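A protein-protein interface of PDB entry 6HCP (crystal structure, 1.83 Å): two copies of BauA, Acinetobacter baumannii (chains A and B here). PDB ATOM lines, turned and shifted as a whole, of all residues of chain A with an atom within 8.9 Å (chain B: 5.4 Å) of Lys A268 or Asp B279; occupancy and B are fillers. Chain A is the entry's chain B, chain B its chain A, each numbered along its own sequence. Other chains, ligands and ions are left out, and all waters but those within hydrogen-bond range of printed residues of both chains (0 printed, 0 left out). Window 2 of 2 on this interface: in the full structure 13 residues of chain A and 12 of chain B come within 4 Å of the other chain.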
ATOM      1  N   VAL A 260     -12.863   9.126 -23.385  1.00  0.00           N
ATOM      2  CA  VAL A 260     -13.005   8.784 -21.988  1.00  0.00           C
ATOM      3  C   VAL A 260     -13.757   9.919 -21.293  1.00  0.00           C
ATOM      4  O   VAL A 260     -13.757  11.053 -21.768  1.00  0.00           O
ATOM      5  CB  VAL A 260     -11.645   8.512 -21.325  1.00  0.00           C
ATOM      6  CG1 VAL A 260     -11.058   7.195 -21.799  1.00  0.00           C
ATOM      7  CG2 VAL A 260     -10.650   9.644 -21.556  1.00  0.00           C
ATOM      8  N   GLY A 265     -13.407   7.099 -16.196  1.00  0.00           N
ATOM      9  CA  GLY A 265     -11.971   7.071 -16.015  1.00  0.00           C
ATOM     10  C   GLY A 265     -11.248   6.435 -17.199  1.00  0.00           C
ATOM     11  O   GLY A 265     -11.869   5.841 -18.083  1.00  0.00           O
ATOM     12  N   ILE A 266      -9.916   6.476 -17.128  1.00  0.00           N
ATOM     13  CA  ILE A 266      -9.027   5.894 -18.128  1.00  0.00           C
ATOM     14  C   ILE A 266      -8.582   4.539 -17.602  1.00  0.00           C
ATOM     15  O   ILE A 266      -7.907   4.473 -16.586  1.00  0.00           O
ATOM     16  CB  ILE A 266      -7.814   6.802 -18.395  1.00  0.00           C
ATOM     17  CG1 ILE A 266      -8.239   8.173 -18.917  1.00  0.00           C
ATOM     18  CG2 ILE A 266      -6.815   6.109 -19.317  1.00  0.00           C
ATOM     19  CD1 ILE A 266      -7.111   9.181 -18.974  1.00  0.00           C
ATOM     20  N   PRO A 267      -8.925   3.433 -18.275  1.00  0.00           N
ATOM     21  CA  PRO A 267      -8.458   2.112 -17.863  1.00  0.00           C
ATOM     22  C   PRO A 267      -7.012   1.873 -18.317  1.00  0.00           C
ATOM     23  O   PRO A 267      -6.462   2.599 -19.151  1.00  0.00           O
ATOM     24  CB  PRO A 267      -9.433   1.195 -18.589  1.00  0.00           C
ATOM     25  CG  PRO A 267      -9.681   1.912 -19.877  1.00  0.00           C
ATOM     26  CD  PRO A 267      -9.687   3.390 -19.524  1.00  0.00           C
ATOM     27  N   LYS A 268      -6.399   0.826 -17.782  1.00  0.00           N
ATOM     28  CA  LYS A 268      -5.046   0.501 -18.163  1.00  0.00           C
ATOM     29  C   LYS A 268      -5.007   0.177 -19.649  1.00  0.00           C
ATOM     30  O   LYS A 268      -5.910  -0.449 -20.187  1.00  0.00           O
ATOM     31  CB  LYS A 268      -4.519  -0.661 -17.329  1.00  0.00           C
ATOM     32  CG  LYS A 268      -4.368  -0.331 -15.851  1.00  0.00           C
ATOM     33  CD  LYS A 268      -3.859  -1.509 -15.049  1.00  0.00           C
ATOM     34  CE  LYS A 268      -4.302  -1.471 -13.602  1.00  0.00           C
ATOM     35  NZ  LYS A 268      -4.009  -0.159 -13.001  1.00  0.00           N
ATOM     36  N   PRO A 269      -3.917   0.550 -20.354  1.00  0.00           N
ATOM     37  CA  PRO A 269      -3.820   0.261 -21.781  1.00  0.00           C
ATOM     38  C   PRO A 269      -3.753  -1.235 -22.058  1.00  0.00           C
ATOM     39  O   PRO A 269      -3.065  -1.974 -21.364  1.00  0.00           O
ATOM     40  CB  PRO A 269      -2.532   0.987 -22.214  1.00  0.00           C
ATOM     41  CG  PRO A 269      -1.730   1.154 -20.927  1.00  0.00           C
ATOM     42  CD  PRO A 269      -2.774   1.327 -19.836  1.00  0.00           C
ATOM     43  N   PRO A 270      -4.511  -1.728 -23.051  1.00  0.00           N
ATOM     44  CA  PRO A 270      -4.329  -3.075 -23.581  1.00  0.00           C
ATOM     45  C   PRO A 270      -2.900  -3.232 -24.109  1.00  0.00           C
ATOM     46  O   PRO A 270      -2.197  -2.218 -24.313  1.00  0.00           O
ATOM     47  CB  PRO A 270      -5.326  -3.158 -24.743  1.00  0.00           C
ATOM     48  CG  PRO A 270      -6.314  -2.059 -24.482  1.00  0.00           C
ATOM     49  CD  PRO A 270      -5.551  -0.972 -23.766  1.00  0.00           C
ATOM     50  N   LYS A 271      -2.536  -4.456 -24.472  1.00  0.00           N
ATOM     51  CA  LYS A 271      -1.217  -4.690 -25.015  1.00  0.00           C
ATOM     52  C   LYS A 271      -1.042  -3.858 -26.292  1.00  0.00           C
ATOM     53  O   LYS A 271      -1.995  -3.586 -27.000  1.00  0.00           O
ATOM     54  CB  LYS A 271      -0.954  -6.176 -25.257  1.00  0.00           C
ATOM     55  CG  LYS A 271      -1.907  -6.898 -26.190  1.00  0.00           C
ATOM     56  CD  LYS A 271      -1.500  -8.355 -26.379  1.00  0.00           C
ATOM     57  CE  LYS A 271      -2.429  -9.128 -27.287  1.00  0.00           C
ATOM     58  NZ  LYS A 271      -2.645  -8.437 -28.582  1.00  0.00           N
ATOM     59  N   THR A 274      -2.680  -4.008 -29.840  1.00  0.00           N
ATOM     60  CA  THR A 274      -4.152  -4.089 -29.915  1.00  0.00           C
ATOM     61  C   THR A 274      -4.676  -3.014 -30.873  1.00  0.00           C
ATOM     62  O   THR A 274      -4.248  -1.867 -30.781  1.00  0.00           O
ATOM     63  CB  THR A 274      -4.796  -3.886 -28.543  1.00  0.00           C
ATOM     64  OG1 THR A 274      -4.256  -4.846 -27.638  1.00  0.00           O
ATOM     65  CG2 THR A 274      -6.310  -3.978 -28.557  1.00  0.00           C
ATOM     66  N   LEU A 276      -7.967  -0.869 -31.515  1.00  0.00           N
ATOM     67  CA  LEU A 276      -9.187  -0.500 -30.808  1.00  0.00           C
ATOM     68  C   LEU A 276     -10.190   0.209 -31.730  1.00  0.00           C
ATOM     69  O   LEU A 276     -11.156   0.818 -31.269  1.00  0.00           O
ATOM     70  CB  LEU A 276      -8.798   0.407 -29.647  1.00  0.00           C
ATOM     71  CG  LEU A 276      -8.028  -0.267 -28.511  1.00  0.00           C
ATOM     72  CD1 LEU A 276      -7.774   0.735 -27.412  1.00  0.00           C
ATOM     73  CD2 LEU A 276      -8.801  -1.460 -27.984  1.00  0.00           C
ATOM     74  N   ILE A 325     -15.036   4.687 -24.137  1.00  0.00           N
ATOM     75  CA  ILE A 325     -14.905   3.732 -23.035  1.00  0.00           C
ATOM     76  C   ILE A 325     -16.004   4.045 -22.014  1.00  0.00           C
ATOM     77  O   ILE A 325     -15.981   5.082 -21.392  1.00  0.00           O
ATOM     78  CB  ILE A 325     -13.493   3.778 -22.421  1.00  0.00           C
ATOM     79  CG1 ILE A 325     -12.434   3.368 -23.446  1.00  0.00           C
ATOM     80  CG2 ILE A 325     -13.424   2.902 -21.179  1.00  0.00           C
ATOM     81  CD1 ILE A 325     -11.016   3.506 -22.987  1.00  0.00           C
ATOM     82  N   SER A 327     -17.175   1.816 -19.535  1.00  0.00           N
ATOM     83  CA  SER A 327     -17.044   1.148 -18.230  1.00  0.00           C
ATOM     84  C   SER A 327     -15.561   0.936 -17.885  1.00  0.00           C
ATOM     85  O   SER A 327     -14.740   0.690 -18.763  1.00  0.00           O
ATOM     86  CB  SER A 327     -17.806  -0.157 -18.225  1.00  0.00           C
ATOM     87  OG  SER A 327     -17.529  -0.907 -17.053  1.00  0.00           O
ATOM     88  N   SER A 328     -15.263   0.866 -16.586  1.00  0.00           N
ATOM     89  CA  SER A 328     -13.915   0.551 -16.127  1.00  0.00           C
ATOM     90  C   SER A 328     -13.600  -0.932 -16.354  1.00  0.00           C
ATOM     91  O   SER A 328     -12.433  -1.319 -16.281  1.00  0.00           O
ATOM     92  CB  SER A 328     -13.738   0.891 -14.675  1.00  0.00           C
ATOM     93  OG  SER A 328     -14.645   0.130 -13.900  1.00  0.00           O
ATOM     94  N   THR A 329     -14.587  -1.721 -16.794  1.00  0.00           N
ATOM     95  CA  THR A 329     -14.281  -3.084 -17.215  1.00  0.00           C
ATOM     96  C   THR A 329     -13.624  -3.115 -18.606  1.00  0.00           C
ATOM     97  O   THR A 329     -13.124  -4.173 -19.022  1.00  0.00           O
ATOM     98  CB  THR A 329     -15.510  -3.995 -17.219  1.00  0.00           C
ATOM     99  OG1 THR A 329     -16.383  -3.516 -18.245  1.00  0.00           O
ATOM    100  CG2 THR A 329     -16.199  -4.043 -15.871  1.00  0.00           C
ATOM    101  N   GLY A 330     -13.695  -2.003 -19.346  1.00  0.00           N
ATOM    102  CA  GLY A 330     -13.106  -1.946 -20.676  1.00  0.00           C
ATOM    103  C   GLY A 330     -14.132  -1.921 -21.800  1.00  0.00           C
ATOM    104  O   GLY A 330     -13.769  -1.928 -22.965  1.00  0.00           O
ATOM    105  N   ASN A 394     -15.049  -4.880 -26.064  1.00  0.00           N
ATOM    106  CA  ASN A 394     -14.281  -4.617 -24.869  1.00  0.00           C
ATOM    107  C   ASN A 394     -12.830  -4.445 -25.316  1.00  0.00           C
ATOM    108  O   ASN A 394     -12.345  -5.223 -26.137  1.00  0.00           O
ATOM    109  CB  ASN A 394     -14.491  -5.719 -23.823  1.00  0.00           C
ATOM    110  CG  ASN A 394     -13.732  -5.471 -22.541  1.00  0.00           C
ATOM    111  OD1 ASN A 394     -12.514  -5.554 -22.531  1.00  0.00           O
ATOM    112  ND2 ASN A 394     -14.431  -5.196 -21.452  1.00  0.00           N
ATOM    113  N   ILE A 395     -12.146  -3.424 -24.788  1.00  0.00           N
ATOM    114  CA  ILE A 395     -10.807  -3.077 -25.274  1.00  0.00           C
ATOM    115  C   ILE A 395      -9.823  -4.215 -25.015  1.00  0.00           C
ATOM    116  O   ILE A 395      -8.789  -4.252 -25.656  1.00  0.00           O
ATOM    117  CB  ILE A 395     -10.283  -1.762 -24.670  1.00  0.00           C
ATOM    118  CG1 ILE A 395     -10.099  -1.855 -23.153  1.00  0.00           C
ATOM    119  CG2 ILE A 395     -11.193  -0.614 -25.072  1.00  0.00           C
ATOM    120  CD1 ILE A 395      -9.529  -0.600 -22.528  1.00  0.00           C
ATOM    121  N   TYR A 396     -10.120  -5.094 -24.055  1.00  0.00           N
ATOM    122  CA  TYR A 396      -9.204  -6.181 -23.722  1.00  0.00           C
ATOM    123  C   TYR A 396      -9.564  -7.480 -24.461  1.00  0.00           C
ATOM    124  O   TYR A 396      -8.906  -8.506 -24.280  1.00  0.00           O
ATOM    125  CB  TYR A 396      -9.199  -6.408 -22.209  1.00  0.00           C
ATOM    126  CG  TYR A 396      -8.865  -5.180 -21.403  1.00  0.00           C
ATOM    127  CD1 TYR A 396      -7.617  -4.584 -21.497  1.00  0.00           C
ATOM    128  CD2 TYR A 396      -9.804  -4.580 -20.588  1.00  0.00           C
ATOM    129  CE1 TYR A 396      -7.326  -3.415 -20.825  1.00  0.00           C
ATOM    130  CE2 TYR A 396      -9.519  -3.424 -19.886  1.00  0.00           C
ATOM    131  CZ  TYR A 396      -8.265  -2.843 -19.998  1.00  0.00           C
ATOM    132  OH  TYR A 396      -7.979  -1.693 -19.334  1.00  0.00           O
ATOM    133  N   VAL A 646      -2.510  10.915 -18.497  1.00  0.00           N
ATOM    134  CA  VAL A 646      -1.813   9.692 -18.732  1.00  0.00           C
ATOM    135  C   VAL A 646      -0.368   9.894 -18.315  1.00  0.00           C
ATOM    136  O   VAL A 646       0.173  10.992 -18.449  1.00  0.00           O
ATOM    137  CB  VAL A 646      -1.906   9.220 -20.193  1.00  0.00           C
ATOM    138  CG1 VAL A 646      -3.339   8.853 -20.561  1.00  0.00           C
ATOM    139  CG2 VAL A 646      -1.332  10.246 -21.164  1.00  0.00           C
ATOM    140  N   PRO A 647       0.310   8.836 -17.834  1.00  0.00           N
ATOM    141  CA  PRO A 647       1.660   8.999 -17.291  1.00  0.00           C
ATOM    142  C   PRO A 647       2.694   9.218 -18.405  1.00  0.00           C
ATOM    143  O   PRO A 647       2.441   8.896 -19.583  1.00  0.00           O
ATOM    144  CB  PRO A 647       1.911   7.684 -16.543  1.00  0.00           C
ATOM    145  CG  PRO A 647       0.986   6.694 -17.203  1.00  0.00           C
ATOM    146  CD  PRO A 647      -0.242   7.494 -17.598  1.00  0.00           C
ATOM    147  N   ALA A 680       3.159  -0.619 -23.755  1.00  0.00           N
ATOM    148  CA  ALA A 680       1.771  -0.190 -23.982  1.00  0.00           C
ATOM    149  C   ALA A 680       1.555   1.156 -23.313  1.00  0.00           C
ATOM    150  O   ALA A 680       1.720   1.274 -22.094  1.00  0.00           O
ATOM    151  CB  ALA A 680       0.808  -1.198 -23.406  1.00  0.00           C
ATOM    152  N   TYR A 681       1.113   2.164 -24.084  1.00  0.00           N
ATOM    153  CA  TYR A 681       0.803   3.455 -23.507  1.00  0.00           C
ATOM    154  C   TYR A 681      -0.301   4.159 -24.301  1.00  0.00           C
ATOM    155  O   TYR A 681      -0.451   3.932 -25.502  1.00  0.00           O
ATOM    156  CB  TYR A 681       2.043   4.363 -23.449  1.00  0.00           C
ATOM    157  CG  TYR A 681       2.622   4.728 -24.792  1.00  0.00           C
ATOM    158  CD1 TYR A 681       3.541   3.904 -25.422  1.00  0.00           C
ATOM    159  CD2 TYR A 681       2.285   5.921 -25.417  1.00  0.00           C
ATOM    160  CE1 TYR A 681       4.050   4.210 -26.674  1.00  0.00           C
ATOM    161  CE2 TYR A 681       2.804   6.255 -26.657  1.00  0.00           C
ATOM    162  CZ  TYR A 681       3.706   5.409 -27.277  1.00  0.00           C
ATOM    163  OH  TYR A 681       4.229   5.707 -28.503  1.00  0.00           O
ATOM    164  N   TRP A 682      -1.069   4.980 -23.578  1.00  0.00           N
ATOM    165  CA  TRP A 682      -2.043   5.889 -24.125  1.00  0.00           C
ATOM    166  C   TRP A 682      -1.331   7.207 -24.418  1.00  0.00           C
ATOM    167  O   TRP A 682      -0.590   7.715 -23.577  1.00  0.00           O
ATOM    168  CB  TRP A 682      -3.205   6.149 -23.166  1.00  0.00           C
ATOM    169  CG  TRP A 682      -4.038   4.972 -22.771  1.00  0.00           C
ATOM    170  CD1 TRP A 682      -4.295   4.581 -21.489  1.00  0.00           C
ATOM    171  CD2 TRP A 682      -5.000   4.296 -23.593  1.00  0.00           C
ATOM    172  NE1 TRP A 682      -5.251   3.602 -21.477  1.00  0.00           N
ATOM    173  CE2 TRP A 682      -5.702   3.403 -22.751  1.00  0.00           C
ATOM    174  CE3 TRP A 682      -5.258   4.261 -24.967  1.00  0.00           C
ATOM    175  CZ2 TRP A 682      -6.738   2.608 -23.223  1.00  0.00           C
ATOM    176  CZ3 TRP A 682      -6.273   3.461 -25.434  1.00  0.00           C
ATOM    177  CH2 TRP A 682      -6.961   2.601 -24.583  1.00  0.00           C
ATOM    178  N   LEU A 690      -7.734   9.496 -26.774  1.00  0.00           N
ATOM    179  CA  LEU A 690      -6.647   8.551 -26.533  1.00  0.00           C
ATOM    180  C   LEU A 690      -6.459   7.655 -27.753  1.00  0.00           C
ATOM    181  O   LEU A 690      -7.431   7.222 -28.384  1.00  0.00           O
ATOM    182  CB  LEU A 690      -6.963   7.630 -25.343  1.00  0.00           C
ATOM    183  CG  LEU A 690      -7.225   8.265 -23.989  1.00  0.00           C
ATOM    184  CD1 LEU A 690      -7.610   7.164 -22.999  1.00  0.00           C
ATOM    185  CD2 LEU A 690      -6.016   9.031 -23.497  1.00  0.00           C
ATOM    186  N   LEU A 692      -3.587   4.108 -28.539  1.00  0.00           N
ATOM    187  CA  LEU A 692      -2.387   3.354 -28.148  1.00  0.00           C
ATOM    188  C   LEU A 692      -1.200   3.743 -29.031  1.00  0.00           C
ATOM    189  O   LEU A 692      -1.319   3.821 -30.269  1.00  0.00           O
ATOM    190  CB  LEU A 692      -2.655   1.856 -28.276  1.00  0.00           C
ATOM    191  CG  LEU A 692      -3.515   1.226 -27.188  1.00  0.00           C
ATOM    192  CD1 LEU A 692      -3.783  -0.232 -27.535  1.00  0.00           C
ATOM    193  CD2 LEU A 692      -2.831   1.342 -25.839  1.00  0.00           C
ATOM    194  N   ASP B 219       2.156  -1.022 -12.948  1.00  0.00           N
ATOM    195  CA  ASP B 219       1.761  -0.102 -11.877  1.00  0.00           C
ATOM    196  C   ASP B 219       2.669  -0.251 -10.642  1.00  0.00           C
ATOM    197  O   ASP B 219       2.292   0.152  -9.545  1.00  0.00           O
ATOM    198  CB  ASP B 219       0.337  -0.367 -11.398  1.00  0.00           C
ATOM    199  CG  ASP B 219      -0.723   0.002 -12.420  1.00  0.00           C
ATOM    200  OD1 ASP B 219      -0.437   0.893 -13.255  1.00  0.00           O
ATOM    201  OD2 ASP B 219      -1.772  -0.693 -12.447  1.00  0.00           O
ATOM    202  N   ASP B 252       5.916   1.464  -4.714  1.00  0.00           N
ATOM    203  CA  ASP B 252       4.500   1.674  -4.989  1.00  0.00           C
ATOM    204  C   ASP B 252       4.031   0.513  -5.868  1.00  0.00           C
ATOM    205  O   ASP B 252       4.739   0.122  -6.779  1.00  0.00           O
ATOM    206  CB  ASP B 252       4.266   3.017  -5.692  1.00  0.00           C
ATOM    207  CG  ASP B 252       4.466   4.243  -4.806  1.00  0.00           C
ATOM    208  OD1 ASP B 252       4.075   4.189  -3.635  1.00  0.00           O
ATOM    209  OD2 ASP B 252       5.071   5.221  -5.281  1.00  0.00           O
ATOM    210  N   GLY B 253       2.875  -0.064  -5.541  1.00  0.00           N
ATOM    211  CA  GLY B 253       2.439  -1.303  -6.144  1.00  0.00           C
ATOM    212  C   GLY B 253       3.241  -2.481  -5.621  1.00  0.00           C
ATOM    213  O   GLY B 253       3.734  -3.328  -6.390  1.00  0.00           O
ATOM    214  N   LEU B 275       0.340  -7.357 -11.549  1.00  0.00           N
ATOM    215  CA  LEU B 275       0.396  -7.065 -10.127  1.00  0.00           C
ATOM    216  C   LEU B 275      -0.917  -7.531  -9.493  1.00  0.00           C
ATOM    217  O   LEU B 275      -1.981  -7.049  -9.836  1.00  0.00           O
ATOM    218  CB  LEU B 275       0.590  -5.564  -9.917  1.00  0.00           C
ATOM    219  CG  LEU B 275       0.635  -5.143  -8.454  1.00  0.00           C
ATOM    220  CD1 LEU B 275       1.808  -5.802  -7.735  1.00  0.00           C
ATOM    221  CD2 LEU B 275       0.687  -3.634  -8.326  1.00  0.00           C
ATOM    222  N   SER B 277      -1.711  -7.368  -6.271  1.00  0.00           N
ATOM    223  CA  SER B 277      -1.981  -6.615  -5.062  1.00  0.00           C
ATOM    224  C   SER B 277      -2.436  -5.217  -5.468  1.00  0.00           C
ATOM    225  O   SER B 277      -2.189  -4.798  -6.599  1.00  0.00           O
ATOM    226  CB  SER B 277      -0.721  -6.570  -4.173  1.00  0.00           C
ATOM    227  OG  SER B 277      -0.253  -7.882  -3.854  1.00  0.00           O
ATOM    228  N   PRO B 278      -3.015  -4.419  -4.549  1.00  0.00           N
ATOM    229  CA  PRO B 278      -3.521  -3.094  -4.903  1.00  0.00           C
ATOM    230  C   PRO B 278      -2.475  -2.205  -5.587  1.00  0.00           C
ATOM    231  O   PRO B 278      -1.361  -2.053  -5.099  1.00  0.00           O
ATOM    232  CB  PRO B 278      -3.965  -2.501  -3.556  1.00  0.00           C
ATOM    233  CG  PRO B 278      -4.287  -3.702  -2.692  1.00  0.00           C
ATOM    234  CD  PRO B 278      -3.380  -4.811  -3.178  1.00  0.00           C
ATOM    235  N   ASP B 279      -2.881  -1.552  -6.692  1.00  0.00           N
ATOM    236  CA  ASP B 279      -2.019  -0.636  -7.413  1.00  0.00           C
ATOM    237  C   ASP B 279      -1.630   0.527  -6.499  1.00  0.00           C
ATOM    238  O   ASP B 279      -0.508   1.009  -6.588  1.00  0.00           O
ATOM    239  CB  ASP B 279      -2.622  -0.164  -8.755  1.00  0.00           C
ATOM    240  CG  ASP B 279      -4.089   0.244  -8.731  1.00  0.00           C
ATOM    241  OD1 ASP B 279      -4.567   0.650  -7.646  1.00  0.00           O
ATOM    242  OD2 ASP B 279      -4.748   0.175  -9.810  1.00  0.00           O
ATOM    243  N   TRP B 280      -2.495   0.871  -5.541  1.00  0.00           N
ATOM    244  CA  TRP B 280      -2.218   1.982  -4.620  1.00  0.00           C
ATOM    245  C   TRP B 280      -1.365   1.546  -3.418  1.00  0.00           C
ATOM    246  O   TRP B 280      -0.937   2.396  -2.640  1.00  0.00           O
ATOM    247  CB  TRP B 280      -3.518   2.638  -4.157  1.00  0.00           C
ATOM    248  CG  TRP B 280      -4.545   1.711  -3.589  1.00  0.00           C
ATOM    249  CD1 TRP B 280      -5.720   1.339  -4.182  1.00  0.00           C
ATOM    250  CD2 TRP B 280      -4.552   1.107  -2.279  1.00  0.00           C
ATOM    251  NE1 TRP B 280      -6.432   0.523  -3.347  1.00  0.00           N
ATOM    252  CE2 TRP B 280      -5.755   0.387  -2.163  1.00  0.00           C
ATOM    253  CE3 TRP B 280      -3.688   1.152  -1.177  1.00  0.00           C
ATOM    254  CZ2 TRP B 280      -6.090  -0.329  -1.018  1.00  0.00           C
ATOM    255  CZ3 TRP B 280      -4.011   0.433  -0.054  1.00  0.00           C
ATOM    256  CH2 TRP B 280      -5.203  -0.282   0.035  1.00  0.00           C
ATOM    257  N   GLY B 281      -1.146   0.236  -3.253  1.00  0.00           N
ATOM    258  CA  GLY B 281      -0.416  -0.279  -2.068  1.00  0.00           C
ATOM    259  C   GLY B 281       1.036   0.152  -2.094  1.00  0.00           C
ATOM    260  O   GLY B 281       1.635   0.266  -3.170  1.00  0.00           O
ATOM    261  N   PRO B 398      -7.337  -7.188 -16.711  1.00  0.00           N
ATOM    262  CA  PRO B 398      -6.265  -6.243 -17.028  1.00  0.00           C
ATOM    263  C   PRO B 398      -6.503  -4.890 -16.367  1.00  0.00           C
ATOM    264  O   PRO B 398      -5.598  -4.095 -16.320  1.00  0.00           O
ATOM    265  CB  PRO B 398      -6.283  -6.130 -18.564  1.00  0.00           C
ATOM    266  CG  PRO B 398      -7.102  -7.315 -19.014  1.00  0.00           C
ATOM    267  CD  PRO B 398      -8.099  -7.567 -17.906  1.00  0.00           C
ATOM    268  N   ASN B 399      -7.724  -4.648 -15.862  1.00  0.00           N
ATOM    269  CA  ASN B 399      -8.049  -3.359 -15.300  1.00  0.00           C
ATOM    270  C   ASN B 399      -8.813  -3.534 -13.992  1.00  0.00           C
ATOM    271  O   ASN B 399      -9.898  -2.973 -13.822  1.00  0.00           O
ATOM    272  CB  ASN B 399      -8.868  -2.484 -16.256  1.00  0.00           C
ATOM    273  CG  ASN B 399      -8.863  -1.039 -15.824  1.00  0.00           C
ATOM    274  OD1 ASN B 399      -7.799  -0.492 -15.550  1.00  0.00           O
ATOM    275  ND2 ASN B 399     -10.036  -0.432 -15.679  1.00  0.00           N
ATOM    276  N   PRO B 400      -8.190  -4.144 -12.958  1.00  0.00           N
ATOM    277  CA  PRO B 400      -8.891  -4.349 -11.690  1.00  0.00           C
ATOM    278  C   PRO B 400      -9.231  -3.018 -11.009  1.00  0.00           C
ATOM    279  O   PRO B 400      -8.466  -2.065 -11.046  1.00  0.00           O
ATOM    280  CB  PRO B 400      -7.877  -5.187 -10.896  1.00  0.00           C
ATOM    281  CG  PRO B 400      -6.540  -4.689 -11.404  1.00  0.00           C
ATOM    282  CD  PRO B 400      -6.776  -4.548 -12.898  1.00  0.00           C
ATOM    283  N   TRP B 402      -9.259  -1.445  -7.592  1.00  0.00           N
ATOM    284  CA  TRP B 402      -8.715  -1.674  -6.251  1.00  0.00           C
ATOM    285  C   TRP B 402      -9.352  -0.720  -5.233  1.00  0.00           C
ATOM    286  O   TRP B 402      -9.073  -0.817  -4.036  1.00  0.00           O
ATOM    287  CB  TRP B 402      -7.190  -1.549  -6.254  1.00  0.00           C
ATOM    288  CG  TRP B 402      -6.513  -2.723  -6.882  1.00  0.00           C
ATOM    289  CD1 TRP B 402      -5.850  -2.749  -8.077  1.00  0.00           C
ATOM    290  CD2 TRP B 402      -6.495  -4.062  -6.374  1.00  0.00           C
ATOM    291  NE1 TRP B 402      -5.399  -4.020  -8.331  1.00  0.00           N
ATOM    292  CE2 TRP B 402      -5.814  -4.850  -7.323  1.00  0.00           C
ATOM    293  CE3 TRP B 402      -6.925  -4.656  -5.180  1.00  0.00           C
ATOM    294  CZ2 TRP B 402      -5.524  -6.192  -7.091  1.00  0.00           C
ATOM    295  CZ3 TRP B 402      -6.641  -5.982  -4.960  1.00  0.00           C
ATOM    296  CH2 TRP B 402      -5.958  -6.741  -5.910  1.00  0.00           C
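Of the 25 printed residues of chain A, 4 touch a printed residue of chain B. Printed residues of chain A that touch a printed residue of chain B: Pro A267, Lys A268, Ser A328 and Tyr A396. Hydrophobic or aromatic side chains of chain A within 4 Å of the printed part of chain B: Pro A267 and Tyr A396. Of the 13 printed residues of chain B, 4 touch a printed residue of chain A. Among the printed residues, 8 pairs touch across the chains.
Of the printed residues of chain B, Lys A268 touches Asp B219 (2.4 Å), Asp B279 (3.3 Å), Pro B398 (3.4 Å) and Asn B399 (2.9 Å). Of the printed residues of chain B, Ser A328 touches Asn B399 (2.6 Å). No residue of chain A comes within 4 Å of Pro B278. Of chain A, only Lys A268 comes within 4 Å of Asp B279. No residue of chain A comes within 4 Å of Gly B281. Of the printed residues of chain A, Pro B398 touches Lys A268 and Tyr A396. The nearest residue of chain A that does not touch Asp B279 is Ile A266 (8.6 Å). The nearest printed residue of chain A that does not touch Asp B219 is Pro A269 (7.0 Å).
The side-chain amino group (NZ) of Lys A268 lies within salt-bridge range of the side-chain carboxylate (OD1) of Asp B219 (3.7 Å). OD2 of Asp B279 is in salt-bridge range of NZ of Lys A268 (3.3 Å). N of Lys A268 lies within hydrogen-bond range of OD1 of Asn B399, 2.9 Å away. The side-chain amide nitrogen of Asn B399 is in hydrogen-bond range of the backbone carbonyl oxygen of Ser A328, 2.6 Å away.
Among the printed residues, pairs that only touch across the chains: Pro A267 with Asn B399, Lys A268 with Pro B398, Tyr A396 with Pro B398 and Tyr A396 with Asn B399.
O of Pro A267 is in hydrogen-bond range of NE1 of Trp A682 (2.8 Å). OH of Tyr A396 lies within hydrogen-bond range of O of Lys A268 (2.6 Å). The backbone NH of Tyr A396 sits at hydrogen-bond distance from the side-chain amide oxygen of Asn A394 (2.9 Å).
No position is printed for both chains. Of the 8 pairs that touch across the chains among the printed residues, none has its exchanged pair printed and touching as well.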
